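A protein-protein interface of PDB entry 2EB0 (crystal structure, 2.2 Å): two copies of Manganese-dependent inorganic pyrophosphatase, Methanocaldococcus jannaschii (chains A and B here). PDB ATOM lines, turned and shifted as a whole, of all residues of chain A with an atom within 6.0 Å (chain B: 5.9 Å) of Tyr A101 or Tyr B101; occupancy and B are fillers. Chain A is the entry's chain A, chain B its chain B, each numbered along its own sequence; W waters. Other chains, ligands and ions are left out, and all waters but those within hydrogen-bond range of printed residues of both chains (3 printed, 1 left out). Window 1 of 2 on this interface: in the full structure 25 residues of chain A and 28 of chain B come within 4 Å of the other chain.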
ATOM      1  N   HIS A  67      19.749  22.534 -22.786  1.00  0.00           N
ATOM      2  CA  HIS A  67      20.410  22.000 -23.969  1.00  0.00           C
ATOM      3  C   HIS A  67      19.590  20.928 -24.671  1.00  0.00           C
ATOM      4  O   HIS A  67      18.740  20.286 -24.062  1.00  0.00           O
ATOM      5  CB  HIS A  67      21.819  21.464 -23.638  1.00  0.00           C
ATOM      6  CG  HIS A  67      21.838  20.155 -22.904  1.00  0.00           C
ATOM      7  ND1 HIS A  67      21.401  20.018 -21.603  1.00  0.00           N
ATOM      8  CD2 HIS A  67      22.267  18.927 -23.287  1.00  0.00           C
ATOM      9  CE1 HIS A  67      21.559  18.763 -21.217  1.00  0.00           C
ATOM     10  NE2 HIS A  67      22.083  18.080 -22.222  1.00  0.00           N
ATOM     11  N   SER A  68      19.838  20.764 -25.966  1.00  0.00           N
ATOM     12  CA  SER A  68      19.148  19.760 -26.756  1.00  0.00           C
ATOM     13  C   SER A  68      20.071  19.379 -27.895  1.00  0.00           C
ATOM     14  O   SER A  68      19.781  19.615 -29.065  1.00  0.00           O
ATOM     15  CB  SER A  68      17.812  20.288 -27.299  1.00  0.00           C
ATOM     16  OG  SER A  68      18.000  21.343 -28.216  1.00  0.00           O
ATOM     17  N   ILE A  83      12.753  12.041 -19.788  1.00  0.00           N
ATOM     18  CA  ILE A  83      11.433  12.461 -19.307  1.00  0.00           C
ATOM     19  C   ILE A  83      11.056  13.841 -19.836  1.00  0.00           C
ATOM     20  O   ILE A  83       9.909  14.088 -20.210  1.00  0.00           O
ATOM     21  CB  ILE A  83      11.389  12.554 -17.761  1.00  0.00           C
ATOM     22  CG1 ILE A  83      11.586  11.177 -17.138  1.00  0.00           C
ATOM     23  CG2 ILE A  83      10.066  13.133 -17.309  1.00  0.00           C
ATOM     24  CD1 ILE A  83      11.648  11.227 -15.629  1.00  0.00           C
ATOM     25  N   ALA A  84      12.028  14.743 -19.858  1.00  0.00           N
ATOM     26  CA  ALA A  84      11.755  16.091 -20.296  1.00  0.00           C
ATOM     27  C   ALA A  84      12.994  16.890 -20.663  1.00  0.00           C
ATOM     28  O   ALA A  84      14.126  16.509 -20.353  1.00  0.00           O
ATOM     29  CB  ALA A  84      10.981  16.820 -19.203  1.00  0.00           C
ATOM     30  N   ILE A  85      12.736  18.006 -21.334  1.00  0.00           N
ATOM     31  CA  ILE A  85      13.745  18.955 -21.761  1.00  0.00           C
ATOM     32  C   ILE A  85      13.104  20.323 -21.589  1.00  0.00           C
ATOM     33  O   ILE A  85      12.040  20.594 -22.135  1.00  0.00           O
ATOM     34  CB  ILE A  85      14.134  18.780 -23.254  1.00  0.00           C
ATOM     35  CG1 ILE A  85      14.723  17.392 -23.493  1.00  0.00           C
ATOM     36  CG2 ILE A  85      15.151  19.829 -23.656  1.00  0.00           C
ATOM     37  CD1 ILE A  85      15.027  17.113 -24.963  1.00  0.00           C
ATOM     38  N   ILE A  86      13.741  21.159 -20.782  1.00  0.00           N
ATOM     39  CA  ILE A  86      13.296  22.518 -20.534  1.00  0.00           C
ATOM     40  C   ILE A  86      14.522  23.276 -21.028  1.00  0.00           C
ATOM     41  O   ILE A  86      15.625  23.103 -20.497  1.00  0.00           O
ATOM     42  CB  ILE A  86      13.088  22.770 -19.046  1.00  0.00           C
ATOM     43  CG1 ILE A  86      12.204  21.670 -18.448  1.00  0.00           C
ATOM     44  CG2 ILE A  86      12.481  24.144 -18.847  1.00  0.00           C
ATOM     45  CD1 ILE A  86      10.837  21.516 -19.113  1.00  0.00           C
ATOM     46  N   ASP A  87      14.340  24.119 -22.034  1.00  0.00           N
ATOM     47  CA  ASP A  87      15.493  24.783 -22.618  1.00  0.00           C
ATOM     48  C   ASP A  87      15.119  26.068 -23.353  1.00  0.00           C
ATOM     49  O   ASP A  87      13.947  26.453 -23.395  1.00  0.00           O
ATOM     50  CB  ASP A  87      16.122  23.778 -23.585  1.00  0.00           C
ATOM     51  CG  ASP A  87      17.398  24.259 -24.193  1.00  0.00           C
ATOM     52  OD1 ASP A  87      17.694  23.812 -25.319  1.00  0.00           O
ATOM     53  OD2 ASP A  87      18.106  25.056 -23.553  1.00  0.00           O
ATOM     54  N   HIS A  89      17.274  26.827 -26.321  1.00  0.00           N
ATOM     55  CA  HIS A  89      18.065  26.700 -27.535  1.00  0.00           C
ATOM     56  C   HIS A  89      17.183  26.134 -28.646  1.00  0.00           C
ATOM     57  O   HIS A  89      16.020  25.806 -28.426  1.00  0.00           O
ATOM     58  CB  HIS A  89      19.247  25.747 -27.320  1.00  0.00           C
ATOM     59  CG  HIS A  89      20.266  26.249 -26.346  1.00  0.00           C
ATOM     60  ND1 HIS A  89      20.081  26.200 -24.981  1.00  0.00           N
ATOM     61  CD2 HIS A  89      21.475  26.828 -26.541  1.00  0.00           C
ATOM     62  CE1 HIS A  89      21.131  26.729 -24.378  1.00  0.00           C
ATOM     63  NE2 HIS A  89      21.992  27.117 -25.302  1.00  0.00           N
ATOM     64  N   LYS A  90      17.748  26.028 -29.841  1.00  0.00           N
ATOM     65  CA  LYS A  90      17.043  25.473 -30.985  1.00  0.00           C
ATOM     66  C   LYS A  90      16.922  23.987 -30.698  1.00  0.00           C
ATOM     67  O   LYS A  90      17.702  23.439 -29.918  1.00  0.00           O
ATOM     68  CB  LYS A  90      17.854  25.692 -32.268  1.00  0.00           C
ATOM     69  CG  LYS A  90      19.223  25.020 -32.273  1.00  0.00           C
ATOM     70  CD  LYS A  90      20.099  25.591 -33.380  1.00  0.00           C
ATOM     71  CE  LYS A  90      21.490  24.986 -33.379  1.00  0.00           C
ATOM     72  NZ  LYS A  90      21.498  23.597 -33.904  1.00  0.00           N
ATOM     73  N   VAL A  91      15.942  23.339 -31.315  1.00  0.00           N
ATOM     74  CA  VAL A  91      15.735  21.915 -31.111  1.00  0.00           C
ATOM     75  C   VAL A  91      16.854  21.163 -31.812  1.00  0.00           C
ATOM     76  O   VAL A  91      16.980  21.233 -33.033  1.00  0.00           O
ATOM     77  CB  VAL A  91      14.386  21.462 -31.704  1.00  0.00           C
ATOM     78  CG1 VAL A  91      14.153  19.986 -31.392  1.00  0.00           C
ATOM     79  CG2 VAL A  91      13.257  22.333 -31.155  1.00  0.00           C
ATOM     80  N   GLY A  92      17.672  20.454 -31.039  1.00  0.00           N
ATOM     81  CA  GLY A  92      18.767  19.706 -31.628  1.00  0.00           C
ATOM     82  C   GLY A  92      18.715  18.231 -31.282  1.00  0.00           C
ATOM     83  O   GLY A  92      19.436  17.417 -31.857  1.00  0.00           O
ATOM     84  N   LEU A  93      17.855  17.883 -30.333  1.00  0.00           N
ATOM     85  CA  LEU A  93      17.713  16.497 -29.911  1.00  0.00           C
ATOM     86  C   LEU A  93      16.424  15.883 -30.438  1.00  0.00           C
ATOM     87  O   LEU A  93      15.383  16.533 -30.474  1.00  0.00           O
ATOM     88  CB  LEU A  93      17.713  16.406 -28.384  1.00  0.00           C
ATOM     89  CG  LEU A  93      18.907  15.743 -27.701  1.00  0.00           C
ATOM     90  CD1 LEU A  93      18.562  15.487 -26.235  1.00  0.00           C
ATOM     91  CD2 LEU A  93      19.239  14.423 -28.392  1.00  0.00           C
ATOM     92  N   THR A  95      13.854  12.378 -30.170  1.00  0.00           N
ATOM     93  CA  THR A  95      13.507  11.333 -29.206  1.00  0.00           C
ATOM     94  C   THR A  95      12.683  10.211 -29.849  1.00  0.00           C
ATOM     95  O   THR A  95      12.123  10.374 -30.939  1.00  0.00           O
ATOM     96  CB  THR A  95      12.700  11.914 -28.015  1.00  0.00           C
ATOM     97  OG1 THR A  95      11.393  12.296 -28.462  1.00  0.00           O
ATOM     98  CG2 THR A  95      13.400  13.146 -27.453  1.00  0.00           C
ATOM     99  N   ILE A  99       7.893  13.133 -24.958  1.00  0.00           N
ATOM    100  CA  ILE A  99       8.479  13.629 -23.727  1.00  0.00           C
ATOM    101  C   ILE A  99       7.855  14.980 -23.462  1.00  0.00           C
ATOM    102  O   ILE A  99       7.189  15.540 -24.329  1.00  0.00           O
ATOM    103  CB  ILE A  99      10.020  13.833 -23.841  1.00  0.00           C
ATOM    104  CG1 ILE A  99      10.337  14.798 -24.990  1.00  0.00           C
ATOM    105  CG2 ILE A  99      10.715  12.498 -24.039  1.00  0.00           C
ATOM    106  CD1 ILE A  99      11.753  15.322 -24.977  1.00  0.00           C
ATOM    107  N   LEU A 100       8.051  15.488 -22.255  1.00  0.00           N
ATOM    108  CA  LEU A 100       7.567  16.803 -21.907  1.00  0.00           C
ATOM    109  C   LEU A 100       8.662  17.713 -22.466  1.00  0.00           C
ATOM    110  O   LEU A 100       9.833  17.607 -22.070  1.00  0.00           O
ATOM    111  CB  LEU A 100       7.485  16.953 -20.391  1.00  0.00           C
ATOM    112  CG  LEU A 100       7.214  18.365 -19.865  1.00  0.00           C
ATOM    113  CD1 LEU A 100       5.721  18.642 -19.893  1.00  0.00           C
ATOM    114  CD2 LEU A 100       7.745  18.486 -18.442  1.00  0.00           C
ATOM    115  N   TYR A 101       8.297  18.575 -23.405  1.00  0.00           N
ATOM    116  CA  TYR A 101       9.263  19.483 -23.999  1.00  0.00           C
ATOM    117  C   TYR A 101       8.747  20.907 -23.893  1.00  0.00           C
ATOM    118  O   TYR A 101       7.622  21.213 -24.290  1.00  0.00           O
ATOM    119  CB  TYR A 101       9.495  19.122 -25.468  1.00  0.00           C
ATOM    120  CG  TYR A 101      10.790  19.647 -26.045  1.00  0.00           C
ATOM    121  CD1 TYR A 101      11.021  21.015 -26.184  1.00  0.00           C
ATOM    122  CD2 TYR A 101      11.793  18.767 -26.449  1.00  0.00           C
ATOM    123  CE1 TYR A 101      12.224  21.492 -26.714  1.00  0.00           C
ATOM    124  CE2 TYR A 101      12.994  19.232 -26.977  1.00  0.00           C
ATOM    125  CZ  TYR A 101      13.205  20.589 -27.107  1.00  0.00           C
ATOM    126  OH  TYR A 101      14.398  21.033 -27.623  1.00  0.00           O
ATOM    127  N   TYR A 102       9.570  21.783 -23.336  1.00  0.00           N
ATOM    128  CA  TYR A 102       9.177  23.171 -23.207  1.00  0.00           C
ATOM    129  C   TYR A 102      10.390  24.052 -23.410  1.00  0.00           C
ATOM    130  O   TYR A 102      11.317  24.062 -22.593  1.00  0.00           O
ATOM    131  CB  TYR A 102       8.564  23.441 -21.836  1.00  0.00           C
ATOM    132  CG  TYR A 102       8.034  24.848 -21.689  1.00  0.00           C
ATOM    133  CD1 TYR A 102       7.321  25.457 -22.726  1.00  0.00           C
ATOM    134  CD2 TYR A 102       8.209  25.559 -20.508  1.00  0.00           C
ATOM    135  CE1 TYR A 102       6.799  26.737 -22.583  1.00  0.00           C
ATOM    136  CE2 TYR A 102       7.684  26.842 -20.350  1.00  0.00           C
ATOM    137  CZ  TYR A 102       6.983  27.423 -21.388  1.00  0.00           C
ATOM    138  OH  TYR A 102       6.448  28.681 -21.235  1.00  0.00           O
ATOM    139  N   ALA A 103      10.373  24.778 -24.521  1.00  0.00           N
ATOM    140  CA  ALA A 103      11.437  25.688 -24.872  1.00  0.00           C
ATOM    141  C   ALA A 103      10.804  27.016 -25.299  1.00  0.00           C
ATOM    142  O   ALA A 103       9.665  27.056 -25.773  1.00  0.00           O
ATOM    143  CB  ALA A 103      12.254  25.101 -25.997  1.00  0.00           C
ATOM    144  N   LYS A 104      11.548  28.100 -25.109  1.00  0.00           N
ATOM    145  CA  LYS A 104      11.107  29.442 -25.468  1.00  0.00           C
ATOM    146  C   LYS A 104      12.329  30.207 -25.953  1.00  0.00           C
ATOM    147  O   LYS A 104      13.439  29.991 -25.459  1.00  0.00           O
ATOM    148  CB  LYS A 104      10.525  30.160 -24.251  1.00  0.00           C
ATOM    149  CG  LYS A 104       9.042  30.453 -24.323  1.00  0.00           C
ATOM    150  CD  LYS A 104       8.503  30.755 -22.925  1.00  0.00           C
ATOM    151  CE  LYS A 104       7.072  31.244 -22.955  1.00  0.00           C
ATOM    152  NZ  LYS A 104       6.992  32.667 -23.370  1.00  0.00           N
ATOM    153  N   HIS B  67       2.213  17.422 -34.418  1.00  0.00           N
ATOM    154  CA  HIS B  67       3.253  16.711 -35.138  1.00  0.00           C
ATOM    155  C   HIS B  67       4.585  17.443 -35.071  1.00  0.00           C
ATOM    156  O   HIS B  67       4.642  18.666 -34.917  1.00  0.00           O
ATOM    157  CB  HIS B  67       2.842  16.434 -36.598  1.00  0.00           C
ATOM    158  CG  HIS B  67       2.916  17.625 -37.507  1.00  0.00           C
ATOM    159  ND1 HIS B  67       2.067  18.704 -37.398  1.00  0.00           N
ATOM    160  CD2 HIS B  67       3.713  17.878 -38.576  1.00  0.00           C
ATOM    161  CE1 HIS B  67       2.334  19.572 -38.361  1.00  0.00           C
ATOM    162  NE2 HIS B  67       3.328  19.094 -39.090  1.00  0.00           N
ATOM    163  N   SER B  68       5.653  16.664 -35.162  1.00  0.00           N
ATOM    164  CA  SER B  68       7.007  17.182 -35.099  1.00  0.00           C
ATOM    165  C   SER B  68       7.860  16.313 -36.012  1.00  0.00           C
ATOM    166  O   SER B  68       8.978  15.939 -35.669  1.00  0.00           O
ATOM    167  CB  SER B  68       7.520  17.097 -33.660  1.00  0.00           C
ATOM    168  OG  SER B  68       8.844  17.585 -33.557  1.00  0.00           O
ATOM    169  N   ALA B  84       6.261  28.131 -33.885  1.00  0.00           N
ATOM    170  CA  ALA B  84       6.098  27.285 -32.705  1.00  0.00           C
ATOM    171  C   ALA B  84       5.646  25.870 -33.020  1.00  0.00           C
ATOM    172  O   ALA B  84       5.254  25.558 -34.143  1.00  0.00           O
ATOM    173  CB  ALA B  84       5.083  27.931 -31.733  1.00  0.00           C
ATOM    174  N   ILE B  85       5.717  25.019 -32.005  1.00  0.00           N
ATOM    175  CA  ILE B  85       5.267  23.643 -32.115  1.00  0.00           C
ATOM    176  C   ILE B  85       4.562  23.287 -30.811  1.00  0.00           C
ATOM    177  O   ILE B  85       5.148  23.405 -29.731  1.00  0.00           O
ATOM    178  CB  ILE B  85       6.437  22.660 -32.343  1.00  0.00           C
ATOM    179  CG1 ILE B  85       7.090  22.926 -33.706  1.00  0.00           C
ATOM    180  CG2 ILE B  85       5.923  21.234 -32.285  1.00  0.00           C
ATOM    181  CD1 ILE B  85       8.229  21.980 -34.047  1.00  0.00           C
ATOM    182  N   ILE B  86       3.298  22.884 -30.927  1.00  0.00           N
ATOM    183  CA  ILE B  86       2.469  22.480 -29.796  1.00  0.00           C
ATOM    184  C   ILE B  86       2.058  21.058 -30.149  1.00  0.00           C
ATOM    185  O   ILE B  86       1.260  20.834 -31.067  1.00  0.00           O
ATOM    186  CB  ILE B  86       1.242  23.385 -29.672  1.00  0.00           C
ATOM    187  CG1 ILE B  86       1.698  24.845 -29.571  1.00  0.00           C
ATOM    188  CG2 ILE B  86       0.422  22.991 -28.448  1.00  0.00           C
ATOM    189  CD1 ILE B  86       2.556  25.139 -28.350  1.00  0.00           C
ATOM    190  N   ASP B  87       2.586  20.094 -29.402  1.00  0.00           N
ATOM    191  CA  ASP B  87       2.359  18.697 -29.738  1.00  0.00           C
ATOM    192  C   ASP B  87       2.302  17.739 -28.545  1.00  0.00           C
ATOM    193  O   ASP B  87       2.321  18.155 -27.382  1.00  0.00           O
ATOM    194  CB  ASP B  87       3.507  18.294 -30.665  1.00  0.00           C
ATOM    195  CG  ASP B  87       3.257  17.015 -31.404  1.00  0.00           C
ATOM    196  OD1 ASP B  87       4.237  16.507 -31.980  1.00  0.00           O
ATOM    197  OD2 ASP B  87       2.105  16.522 -31.425  1.00  0.00           O
ATOM    198  N   HIS B  89       3.683  14.336 -29.406  1.00  0.00           N
ATOM    199  CA  HIS B  89       4.410  13.222 -29.998  1.00  0.00           C
ATOM    200  C   HIS B  89       5.866  13.408 -29.611  1.00  0.00           C
ATOM    201  O   HIS B  89       6.217  14.393 -28.961  1.00  0.00           O
ATOM    202  CB  HIS B  89       4.292  13.225 -31.524  1.00  0.00           C
ATOM    203  CG  HIS B  89       2.899  13.018 -32.022  1.00  0.00           C
ATOM    204  ND1 HIS B  89       1.970  14.034 -32.078  1.00  0.00           N
ATOM    205  CD2 HIS B  89       2.266  11.902 -32.458  1.00  0.00           C
ATOM    206  CE1 HIS B  89       0.822  13.554 -32.528  1.00  0.00           C
ATOM    207  NE2 HIS B  89       0.975  12.262 -32.765  1.00  0.00           N
ATOM    208  N   LYS B  90       6.703  12.455 -29.997  1.00  0.00           N
ATOM    209  CA  LYS B  90       8.135  12.518 -29.724  1.00  0.00           C
ATOM    210  C   LYS B  90       8.697  13.696 -30.520  1.00  0.00           C
ATOM    211  O   LYS B  90       8.058  14.169 -31.453  1.00  0.00           O
ATOM    212  CB  LYS B  90       8.810  11.236 -30.215  1.00  0.00           C
ATOM    213  CG  LYS B  90       8.810  11.108 -31.736  1.00  0.00           C
ATOM    214  CD  LYS B  90       9.086   9.679 -32.167  1.00  0.00           C
ATOM    215  CE  LYS B  90       9.296   9.569 -33.669  1.00  0.00           C
ATOM    216  NZ  LYS B  90      10.575  10.204 -34.100  1.00  0.00           N
ATOM    217  N   VAL B  91       9.886  14.167 -30.160  1.00  0.00           N
ATOM    218  CA  VAL B  91      10.492  15.253 -30.913  1.00  0.00           C
ATOM    219  C   VAL B  91      11.115  14.635 -32.170  1.00  0.00           C
ATOM    220  O   VAL B  91      11.933  13.714 -32.083  1.00  0.00           O
ATOM    221  CB  VAL B  91      11.597  15.969 -30.115  1.00  0.00           C
ATOM    222  CG1 VAL B  91      12.251  17.023 -30.995  1.00  0.00           C
ATOM    223  CG2 VAL B  91      11.002  16.614 -28.865  1.00  0.00           C
ATOM    224  N   GLY B  92      10.710  15.126 -33.335  1.00  0.00           N
ATOM    225  CA  GLY B  92      11.248  14.596 -34.573  1.00  0.00           C
ATOM    226  C   GLY B  92      11.757  15.680 -35.501  1.00  0.00           C
ATOM    227  O   GLY B  92      12.203  15.385 -36.604  1.00  0.00           O
ATOM    228  N   LEU B  93      11.692  16.932 -35.056  1.00  0.00           N
ATOM    229  CA  LEU B  93      12.146  18.060 -35.865  1.00  0.00           C
ATOM    230  C   LEU B  93      13.201  18.885 -35.163  1.00  0.00           C
ATOM    231  O   LEU B  93      13.005  19.294 -34.024  1.00  0.00           O
ATOM    232  CB  LEU B  93      10.986  19.011 -36.197  1.00  0.00           C
ATOM    233  CG  LEU B  93       9.960  18.699 -37.287  1.00  0.00           C
ATOM    234  CD1 LEU B  93       9.007  19.881 -37.419  1.00  0.00           C
ATOM    235  CD2 LEU B  93      10.663  18.444 -38.616  1.00  0.00           C
ATOM    236  N   THR B  95      15.433  22.407 -35.250  1.00  0.00           N
ATOM    237  CA  THR B  95      15.181  23.740 -35.776  1.00  0.00           C
ATOM    238  C   THR B  95      16.488  24.512 -35.917  1.00  0.00           C
ATOM    239  O   THR B  95      17.495  24.183 -35.292  1.00  0.00           O
ATOM    240  CB  THR B  95      14.224  24.548 -34.863  1.00  0.00           C
ATOM    241  OG1 THR B  95      14.848  24.769 -33.592  1.00  0.00           O
ATOM    242  CG2 THR B  95      12.897  23.799 -34.669  1.00  0.00           C
ATOM    243  N   ILE B  99      12.873  28.351 -30.718  1.00  0.00           N
ATOM    244  CA  ILE B  99      11.463  28.418 -31.049  1.00  0.00           C
ATOM    245  C   ILE B  99      10.604  28.113 -29.839  1.00  0.00           C
ATOM    246  O   ILE B  99      11.089  27.543 -28.865  1.00  0.00           O
ATOM    247  CB  ILE B  99      11.177  27.383 -32.168  1.00  0.00           C
ATOM    248  CG1 ILE B  99      11.242  28.073 -33.526  1.00  0.00           C
ATOM    249  CG2 ILE B  99       9.871  26.652 -31.922  1.00  0.00           C
ATOM    250  CD1 ILE B  99      11.288  27.115 -34.686  1.00  0.00           C
ATOM    251  N   LEU B 100       9.339  28.524 -29.880  1.00  0.00           N
ATOM    252  CA  LEU B 100       8.431  28.189 -28.794  1.00  0.00           C
ATOM    253  C   LEU B 100       8.097  26.726 -29.082  1.00  0.00           C
ATOM    254  O   LEU B 100       7.593  26.386 -30.161  1.00  0.00           O
ATOM    255  CB  LEU B 100       7.154  29.016 -28.849  1.00  0.00           C
ATOM    256  CG  LEU B 100       6.012  28.445 -27.996  1.00  0.00           C
ATOM    257  CD1 LEU B 100       6.338  28.540 -26.516  1.00  0.00           C
ATOM    258  CD2 LEU B 100       4.747  29.202 -28.295  1.00  0.00           C
ATOM    259  N   TYR B 101       8.406  25.854 -28.135  1.00  0.00           N
ATOM    260  CA  TYR B 101       8.131  24.441 -28.322  1.00  0.00           C
ATOM    261  C   TYR B 101       7.460  23.938 -27.062  1.00  0.00           C
ATOM    262  O   TYR B 101       8.029  24.033 -25.981  1.00  0.00           O
ATOM    263  CB  TYR B 101       9.432  23.681 -28.562  1.00  0.00           C
ATOM    264  CG  TYR B 101       9.234  22.308 -29.141  1.00  0.00           C
ATOM    265  CD1 TYR B 101       8.435  21.362 -28.494  1.00  0.00           C
ATOM    266  CD2 TYR B 101       9.824  21.955 -30.347  1.00  0.00           C
ATOM    267  CE1 TYR B 101       8.228  20.098 -29.039  1.00  0.00           C
ATOM    268  CE2 TYR B 101       9.625  20.694 -30.900  1.00  0.00           C
ATOM    269  CZ  TYR B 101       8.825  19.773 -30.239  1.00  0.00           C
ATOM    270  OH  TYR B 101       8.633  18.528 -30.783  1.00  0.00           O
ATOM    271  N   TYR B 102       6.249  23.411 -27.199  1.00  0.00           N
ATOM    272  CA  TYR B 102       5.534  22.906 -26.037  1.00  0.00           C
ATOM    273  C   TYR B 102       4.840  21.582 -26.331  1.00  0.00           C
ATOM    274  O   TYR B 102       3.860  21.532 -27.088  1.00  0.00           O
ATOM    275  CB  TYR B 102       4.513  23.943 -25.554  1.00  0.00           C
ATOM    276  CG  TYR B 102       3.814  23.561 -24.267  1.00  0.00           C
ATOM    277  CD1 TYR B 102       4.532  23.030 -23.190  1.00  0.00           C
ATOM    278  CD2 TYR B 102       2.438  23.731 -24.120  1.00  0.00           C
ATOM    279  CE1 TYR B 102       3.893  22.677 -22.008  1.00  0.00           C
ATOM    280  CE2 TYR B 102       1.791  23.382 -22.936  1.00  0.00           C
ATOM    281  CZ  TYR B 102       2.522  22.855 -21.885  1.00  0.00           C
ATOM    282  OH  TYR B 102       1.887  22.495 -20.720  1.00  0.00           O
ATOM    283  N   ALA B 103       5.369  20.512 -25.745  1.00  0.00           N
ATOM    284  CA  ALA B 103       4.793  19.181 -25.918  1.00  0.00           C
ATOM    285  C   ALA B 103       4.703  18.416 -24.590  1.00  0.00           C
ATOM    286  O   ALA B 103       5.642  18.404 -23.799  1.00  0.00           O
ATOM    287  CB  ALA B 103       5.611  18.379 -26.947  1.00  0.00           C
ATOM    288  N   LYS B 104       3.552  17.802 -24.338  1.00  0.00           N
ATOM    289  CA  LYS B 104       3.347  17.019 -23.122  1.00  0.00           C
ATOM    290  C   LYS B 104       2.947  15.627 -23.563  1.00  0.00           C
ATOM    291  O   LYS B 104       2.166  15.471 -24.498  1.00  0.00           O
ATOM    292  CB  LYS B 104       2.229  17.610 -22.251  1.00  0.00           C
ATOM    293  CG  LYS B 104       2.539  18.981 -21.677  1.00  0.00           C
ATOM    294  CD  LYS B 104       1.365  19.572 -20.890  1.00  0.00           C
ATOM    295  CE  LYS B 104       1.406  19.233 -19.394  1.00  0.00           C
ATOM    296  NZ  LYS B 104       1.022  17.836 -19.070  1.00  0.00           N
ATOM    297  N   PRO B 105       3.483  14.592 -22.906  1.00  0.00           N
ATOM    298  CA  PRO B 105       3.090  13.248 -23.336  1.00  0.00           C
ATOM    299  C   PRO B 105       1.690  12.846 -22.841  1.00  0.00           C
ATOM    300  O   PRO B 105       1.551  11.942 -22.022  1.00  0.00           O
ATOM    301  CB  PRO B 105       4.207  12.366 -22.777  1.00  0.00           C
ATOM    302  CG  PRO B 105       4.597  13.076 -21.500  1.00  0.00           C
ATOM    303  CD  PRO B 105       4.561  14.554 -21.895  1.00  0.00           C
HETATM  304  O   HOH W   1      19.582  21.831 -34.046  1.00  0.00           O
HETATM  305  O   HOH W   2       7.946  14.789 -27.056  1.00  0.00           O
HETATM  306  O   HOH W   3      13.507  25.657 -29.361  1.00  0.00           O
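Of the 19 printed residues of chain B, 11 touch a printed residue of chain A. Printed residues of chain B that touch a printed residue of chain A: Lys B90, Val B91, Leu B93, Thr B95, Ile B99, Leu B100, Tyr B101, Tyr B102, Ala B103, Lys B104 and Pro B105. Hydrophobic or aromatic side chains of chain B that line the printed part of chain A: Val B91, Leu B100, Tyr B101, Tyr B102 and Pro B105. Hydrophobic or aromatic side chains of chain A that line the printed part of chain B: Val A91, Leu A100, Tyr A101, Tyr A102 and Ala A103.
Tyr A101 touches its own counterpart, Tyr B101. Tyr A101 touches Tyr B102, and with the chains exchanged Tyr A102 touches Tyr B101. Lys A104 touches Ile B99, but with the chains exchanged Ile A99 does not touch Lys B104 (4.3 Å). Of the 24 pairs that touch across the chains among the printed residues, 21 have their exchanged pair printed and touching as well.
The backbone NH (N) of Val A91 lies within hydrogen-bond range of the side-chain hydroxyl (OG1) of Thr B95, at 2.9 Å. The side-chain hydroxyl (OG1) of Thr A95 is in hydrogen-bond range of the backbone NH (N) of Val B91, 2.9 Å away. N of Tyr A101 sits at hydrogen-bond distance from O of Ala B103, 2.7 Å away. The backbone NH (N) of Ala A103 lies within hydrogen-bond range of the backbone carbonyl oxygen (O) of Tyr B101, 2.9 Å away. O of Ile A99 lies close to O of Ala B103 (3.3 Å). O of Tyr B101 lies close to O of Tyr A101 (3.3 Å). The backbone carbonyl oxygen of Ala A103 lies close to the backbone carbonyl oxygen of Ile B99, 3.4 Å away.
O of Thr B95 touches CB of Lys A90, at 3.4 Å. CG1 of Val A91 touches CG1 of Val B91, at 3.5 Å. Tyr B101 touches Val A91. Leu A93 touches Val B91 (O to CG1, 3.2 Å). CA of Leu A100 touches O of Ala B103, at 3.1 Å. CG of Lys B104 touches CD1 of Leu A100, 3.7 Å away. Pro B105 touches Leu A100. CA of Tyr B102 touches O of Tyr A101, at 3.2 Å. Tyr A102 touches Tyr B102. Lys A104 touches Leu B100 (CG to CD1, 3.97 Å).
Water W2 lies within hydrogen-bond range of O of His B89 and N of Ile A99. Water W1 lies within hydrogen-bond range of NZ of Lys A90 (2.6 Å), O of Val A91 (2.9 Å) and O of Thr B95 (3.4 Å). Water W3 bridges the backbone carbonyl oxygen (O) of His A89 (2.7 Å) and the backbone NH (N) of Ile B99 (3.1 Å).
Printed residues of chain B within 4 Å of Lys A90: Thr B95. Of the printed residues of chain B, Lys A104 touches Ile B99 and Leu B100. Tyr B101 touches just these residues of chain A: Val A91 (3.5 Å), Tyr A101 (3.3 Å), Tyr A102 (3.1 Å) and Ala A103 (2.9 Å). The nearest residue of chain B that does not touch Tyr A101 is Lys B104 (4.9 Å). The nearest residue of chain A that does not touch Tyr B101 is Lys A104 (4.9 Å).
O of Lys A90 is in hydrogen-bond range of OG of Ser A68, 2.7 Å away. The backbone carbonyl oxygen of Ser A68 is in hydrogen-bond range of the backbone NH of Leu A93 (2.9 Å). The backbone NH of Asp A87 is in hydrogen-bond range of the backbone carbonyl oxygen of Tyr A102 (3.1 Å). N of Lys A104 is in hydrogen-bond range of O of Asp A87. N of Ile B85 lies within hydrogen-bond range of O of Leu B100, 3.0 Å away.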
